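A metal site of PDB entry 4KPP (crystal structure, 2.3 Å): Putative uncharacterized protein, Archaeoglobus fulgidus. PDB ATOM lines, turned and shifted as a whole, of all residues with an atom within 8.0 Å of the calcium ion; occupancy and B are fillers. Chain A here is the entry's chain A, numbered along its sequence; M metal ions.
The backbone NH (N) of Glu 340 lies close to the side-chain hydroxyl (OG) of Ser 337. The side-chain carboxylate (OD2) of Asp 333 sits close to the side-chain amino group (NZ) of Lys 378, 3.9 Å away.
Four residues have an atom within 4 Å of the calcium ion: Ile 330, Asp 333, Lys 335 and Glu 340. The nearest printed residue that does not touch the calcium ion is Ile 336 (4.1 Å).
The calcium ion is bound by the backbone carbonyl oxygen (O) of Lys 335, at 2.1 Å. OE1 of Glu 340 binds the calcium ion, 2.2 Å away. OD1 of Asp 333 binds the calcium ion (2.4 Å). The calcium ion is bound by the side-chain carboxylate (OE2) of Glu 340 (2.5 Å). O of Ile 330 is bound to the calcium ion, 2.5 Å away. The side-chain carboxylate (OD2) of Asp 333 is bound to the calcium ion. The calcium ion has six donor atoms within binding distance.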
ATOM      1  N   GLU A 131      15.413  33.326 -20.219  1.00  0.00           N
ATOM      2  CA  GLU A 131      16.163  32.974 -21.421  1.00  0.00           C
ATOM      3  C   GLU A 131      17.035  34.126 -21.911  1.00  0.00           C
ATOM      4  O   GLU A 131      16.592  35.282 -21.935  1.00  0.00           O
ATOM      5  CB  GLU A 131      15.220  32.522 -22.539  1.00  0.00           C
ATOM      6  CG  GLU A 131      15.914  32.203 -23.855  1.00  0.00           C
ATOM      7  CD  GLU A 131      14.932  31.918 -24.978  1.00  0.00           C
ATOM      8  OE1 GLU A 131      15.351  31.955 -26.155  1.00  0.00           O
ATOM      9  OE2 GLU A 131      13.740  31.667 -24.690  1.00  0.00           O
ATOM     10  N   VAL A 132      18.278  33.815 -22.295  1.00  0.00           N
ATOM     11  CA  VAL A 132      19.173  34.794 -22.889  1.00  0.00           C
ATOM     12  C   VAL A 132      19.457  34.433 -24.342  1.00  0.00           C
ATOM     13  O   VAL A 132      19.940  33.331 -24.629  1.00  0.00           O
ATOM     14  CB  VAL A 132      20.508  34.890 -22.122  1.00  0.00           C
ATOM     15  CG1 VAL A 132      21.544  35.614 -22.946  1.00  0.00           C
ATOM     16  CG2 VAL A 132      20.301  35.592 -20.790  1.00  0.00           C
ATOM     17  N   LEU A 134      21.350  35.021 -28.090  1.00  0.00           N
ATOM     18  CA  LEU A 134      22.607  35.510 -28.648  1.00  0.00           C
ATOM     19  C   LEU A 134      22.467  35.895 -30.119  1.00  0.00           C
ATOM     20  O   LEU A 134      21.563  35.410 -30.815  1.00  0.00           O
ATOM     21  CB  LEU A 134      23.711  34.454 -28.490  1.00  0.00           C
ATOM     22  CG  LEU A 134      24.141  34.043 -27.081  1.00  0.00           C
ATOM     23  CD1 LEU A 134      24.014  35.193 -26.089  1.00  0.00           C
ATOM     24  CD2 LEU A 134      23.372  32.817 -26.597  1.00  0.00           C
ATOM     25  N   PHE A 326      30.526  20.669 -24.143  1.00  0.00           N
ATOM     26  CA  PHE A 326      29.204  20.927 -23.600  1.00  0.00           C
ATOM     27  C   PHE A 326      28.811  22.390 -23.778  1.00  0.00           C
ATOM     28  O   PHE A 326      27.644  22.703 -24.011  1.00  0.00           O
ATOM     29  CB  PHE A 326      29.175  20.530 -22.125  1.00  0.00           C
ATOM     30  CG  PHE A 326      27.819  20.654 -21.493  1.00  0.00           C
ATOM     31  CD1 PHE A 326      26.738  19.942 -22.007  1.00  0.00           C
ATOM     32  CD2 PHE A 326      27.627  21.468 -20.394  1.00  0.00           C
ATOM     33  CE1 PHE A 326      25.484  20.059 -21.415  1.00  0.00           C
ATOM     34  CE2 PHE A 326      26.385  21.583 -19.805  1.00  0.00           C
ATOM     35  CZ  PHE A 326      25.307  20.879 -20.314  1.00  0.00           C
ATOM     36  N   ALA A 327      29.802  23.281 -23.668  1.00  0.00           N
ATOM     37  CA  ALA A 327      29.577  24.702 -23.881  1.00  0.00           C
ATOM     38  C   ALA A 327      29.171  24.994 -25.320  1.00  0.00           C
ATOM     39  O   ALA A 327      28.221  25.738 -25.571  1.00  0.00           O
ATOM     40  CB  ALA A 327      30.821  25.500 -23.499  1.00  0.00           C
ATOM     41  N   VAL A 328      29.886  24.393 -26.269  1.00  0.00           N
ATOM     42  CA  VAL A 328      29.574  24.531 -27.694  1.00  0.00           C
ATOM     43  C   VAL A 328      28.154  24.060 -27.997  1.00  0.00           C
ATOM     44  O   VAL A 328      27.394  24.750 -28.695  1.00  0.00           O
ATOM     45  CB  VAL A 328      30.558  23.722 -28.556  1.00  0.00           C
ATOM     46  CG1 VAL A 328      30.028  23.565 -29.973  1.00  0.00           C
ATOM     47  CG2 VAL A 328      31.922  24.385 -28.570  1.00  0.00           C
ATOM     48  N   ALA A 329      27.799  22.893 -27.473  1.00  0.00           N
ATOM     49  CA  ALA A 329      26.493  22.306 -27.733  1.00  0.00           C
ATOM     50  C   ALA A 329      25.354  23.186 -27.216  1.00  0.00           C
ATOM     51  O   ALA A 329      24.279  23.249 -27.811  1.00  0.00           O
ATOM     52  CB  ALA A 329      26.402  20.906 -27.119  1.00  0.00           C
ATOM     53  N   ILE A 330      25.602  23.865 -26.104  1.00  0.00           N
ATOM     54  CA  ILE A 330      24.624  24.769 -25.500  1.00  0.00           C
ATOM     55  C   ILE A 330      24.432  26.031 -26.336  1.00  0.00           C
ATOM     56  O   ILE A 330      23.315  26.537 -26.453  1.00  0.00           O
ATOM     57  CB  ILE A 330      25.044  25.141 -24.052  1.00  0.00           C
ATOM     58  CG1 ILE A 330      24.753  23.989 -23.098  1.00  0.00           C
ATOM     59  CG2 ILE A 330      24.336  26.405 -23.579  1.00  0.00           C
ATOM     60  CD1 ILE A 330      25.112  24.277 -21.659  1.00  0.00           C
ATOM     61  N   LEU A 331      25.513  26.521 -26.932  1.00  0.00           N
ATOM     62  CA  LEU A 331      25.458  27.738 -27.736  1.00  0.00           C
ATOM     63  C   LEU A 331      24.787  27.542 -29.095  1.00  0.00           C
ATOM     64  O   LEU A 331      24.428  28.521 -29.758  1.00  0.00           O
ATOM     65  CB  LEU A 331      26.862  28.304 -27.936  1.00  0.00           C
ATOM     66  CG  LEU A 331      27.655  28.653 -26.682  1.00  0.00           C
ATOM     67  CD1 LEU A 331      29.035  29.173 -27.062  1.00  0.00           C
ATOM     68  CD2 LEU A 331      26.905  29.664 -25.817  1.00  0.00           C
ATOM     69  N   LEU A 332      24.629  26.288 -29.517  1.00  0.00           N
ATOM     70  CA  LEU A 332      24.145  25.990 -30.874  1.00  0.00           C
ATOM     71  C   LEU A 332      22.758  26.553 -31.208  1.00  0.00           C
ATOM     72  O   LEU A 332      22.511  26.941 -32.353  1.00  0.00           O
ATOM     73  CB  LEU A 332      24.190  24.480 -31.130  1.00  0.00           C
ATOM     74  CG  LEU A 332      25.558  23.875 -31.412  1.00  0.00           C
ATOM     75  CD1 LEU A 332      25.464  22.364 -31.489  1.00  0.00           C
ATOM     76  CD2 LEU A 332      26.154  24.441 -32.701  1.00  0.00           C
ATOM     77  N   ASP A 333      21.874  26.605 -30.225  1.00  0.00           N
ATOM     78  CA  ASP A 333      20.521  27.142 -30.445  1.00  0.00           C
ATOM     79  C   ASP A 333      20.500  28.670 -30.338  1.00  0.00           C
ATOM     80  O   ASP A 333      19.428  29.283 -30.396  1.00  0.00           O
ATOM     81  CB  ASP A 333      19.512  26.504 -29.491  1.00  0.00           C
ATOM     82  CG  ASP A 333      19.938  26.598 -28.033  1.00  0.00           C
ATOM     83  OD1 ASP A 333      21.021  27.168 -27.776  1.00  0.00           O
ATOM     84  OD2 ASP A 333      19.193  26.106 -27.162  1.00  0.00           O
ATOM     85  N   LEU A 334      21.671  29.274 -30.210  1.00  0.00           N
ATOM     86  CA  LEU A 334      21.823  30.723 -30.052  1.00  0.00           C
ATOM     87  C   LEU A 334      21.029  31.263 -28.867  1.00  0.00           C
ATOM     88  O   LEU A 334      20.554  32.406 -28.894  1.00  0.00           O
ATOM     89  CB  LEU A 334      21.452  31.466 -31.346  1.00  0.00           C
ATOM     90  CG  LEU A 334      22.380  31.243 -32.533  1.00  0.00           C
ATOM     91  CD1 LEU A 334      21.962  32.096 -33.724  1.00  0.00           C
ATOM     92  CD2 LEU A 334      23.812  31.544 -32.142  1.00  0.00           C
ATOM     93  N   LYS A 335      20.884  30.438 -27.836  1.00  0.00           N
ATOM     94  CA  LYS A 335      20.172  30.819 -26.621  1.00  0.00           C
ATOM     95  C   LYS A 335      20.791  30.164 -25.402  1.00  0.00           C
ATOM     96  O   LYS A 335      21.278  29.033 -25.467  1.00  0.00           O
ATOM     97  CB  LYS A 335      18.692  30.445 -26.728  1.00  0.00           C
ATOM     98  N   ILE A 336      20.778  30.872 -24.269  1.00  0.00           N
ATOM     99  CA  ILE A 336      21.251  30.297 -23.011  1.00  0.00           C
ATOM    100  C   ILE A 336      20.105  30.279 -21.999  1.00  0.00           C
ATOM    101  O   ILE A 336      19.704  31.327 -21.489  1.00  0.00           O
ATOM    102  CB  ILE A 336      22.444  31.066 -22.426  1.00  0.00           C
ATOM    103  CG1 ILE A 336      23.601  31.103 -23.436  1.00  0.00           C
ATOM    104  CG2 ILE A 336      22.908  30.419 -21.119  1.00  0.00           C
ATOM    105  CD1 ILE A 336      24.830  31.818 -22.920  1.00  0.00           C
ATOM    106  N   SER A 337      19.582  29.088 -21.727  1.00  0.00           N
ATOM    107  CA  SER A 337      18.449  28.939 -20.826  1.00  0.00           C
ATOM    108  C   SER A 337      18.918  28.793 -19.382  1.00  0.00           C
ATOM    109  O   SER A 337      20.105  28.676 -19.110  1.00  0.00           O
ATOM    110  CB  SER A 337      17.592  27.737 -21.231  1.00  0.00           C
ATOM    111  OG  SER A 337      18.337  26.530 -21.123  1.00  0.00           O
ATOM    112  N   TRP A 338      17.964  28.803 -18.457  1.00  0.00           N
ATOM    113  CA  TRP A 338      18.269  28.716 -17.035  1.00  0.00           C
ATOM    114  C   TRP A 338      18.746  27.307 -16.678  1.00  0.00           C
ATOM    115  O   TRP A 338      19.579  27.135 -15.782  1.00  0.00           O
ATOM    116  CB  TRP A 338      17.059  29.113 -16.184  1.00  0.00           C
ATOM    117  CG  TRP A 338      16.449  27.977 -15.434  1.00  0.00           C
ATOM    118  CD1 TRP A 338      15.516  27.087 -15.895  1.00  0.00           C
ATOM    119  CD2 TRP A 338      16.721  27.605 -14.076  1.00  0.00           C
ATOM    120  NE1 TRP A 338      15.201  26.183 -14.909  1.00  0.00           N
ATOM    121  CE2 TRP A 338      15.919  26.473 -13.788  1.00  0.00           C
ATOM    122  CE3 TRP A 338      17.559  28.108 -13.082  1.00  0.00           C
ATOM    123  CZ2 TRP A 338      15.941  25.847 -12.543  1.00  0.00           C
ATOM    124  CZ3 TRP A 338      17.573  27.487 -11.842  1.00  0.00           C
ATOM    125  CH2 TRP A 338      16.775  26.372 -11.585  1.00  0.00           C
ATOM    126  N   GLU A 340      20.463  25.300 -18.783  1.00  0.00           N
ATOM    127  CA  GLU A 340      21.817  25.197 -19.303  1.00  0.00           C
ATOM    128  C   GLU A 340      22.805  25.963 -18.435  1.00  0.00           C
ATOM    129  O   GLU A 340      23.902  25.479 -18.155  1.00  0.00           O
ATOM    130  CB  GLU A 340      21.871  25.702 -20.750  1.00  0.00           C
ATOM    131  CG  GLU A 340      21.104  24.847 -21.744  1.00  0.00           C
ATOM    132  CD  GLU A 340      21.014  25.478 -23.110  1.00  0.00           C
ATOM    133  OE1 GLU A 340      21.135  26.720 -23.202  1.00  0.00           O
ATOM    134  OE2 GLU A 340      20.819  24.750 -24.100  1.00  0.00           O
ATOM    135  N   ALA A 341      22.416  27.167 -17.999  1.00  0.00           N
ATOM    136  CA  ALA A 341      23.266  27.971 -17.127  1.00  0.00           C
ATOM    137  C   ALA A 341      23.485  27.299 -15.775  1.00  0.00           C
ATOM    138  O   ALA A 341      24.601  27.252 -15.273  1.00  0.00           O
ATOM    139  CB  ALA A 341      22.666  29.361 -16.938  1.00  0.00           C
ATOM    140  N   ILE A 374      22.375  16.622 -27.801  1.00  0.00           N
ATOM    141  CA  ILE A 374      22.203  18.003 -28.224  1.00  0.00           C
ATOM    142  C   ILE A 374      22.848  18.218 -29.584  1.00  0.00           C
ATOM    143  O   ILE A 374      22.214  18.753 -30.494  1.00  0.00           O
ATOM    144  CB  ILE A 374      22.806  18.985 -27.204  1.00  0.00           C
ATOM    145  CG1 ILE A 374      22.128  18.826 -25.840  1.00  0.00           C
ATOM    146  CG2 ILE A 374      22.664  20.424 -27.703  1.00  0.00           C
ATOM    147  CD1 ILE A 374      22.647  19.767 -24.768  1.00  0.00           C
ATOM    148  N   LYS A 378      20.799  19.141 -32.944  1.00  0.00           N
ATOM    149  CA  LYS A 378      21.056  20.468 -33.471  1.00  0.00           C
ATOM    150  C   LYS A 378      22.114  20.415 -34.564  1.00  0.00           C
ATOM    151  O   LYS A 378      22.912  21.347 -34.705  1.00  0.00           O
ATOM    152  CB  LYS A 378      21.518  21.402 -32.356  1.00  0.00           C
ATOM    153  CG  LYS A 378      20.585  21.473 -31.167  1.00  0.00           C
ATOM    154  CD  LYS A 378      19.273  22.155 -31.521  1.00  0.00           C
ATOM    155  CE  LYS A 378      18.316  22.148 -30.351  1.00  0.00           C
ATOM    156  NZ  LYS A 378      18.954  22.680 -29.112  1.00  0.00           N
HETATM  157 CA    CA M   1      21.041  26.899 -25.367  1.00  0.00          CA
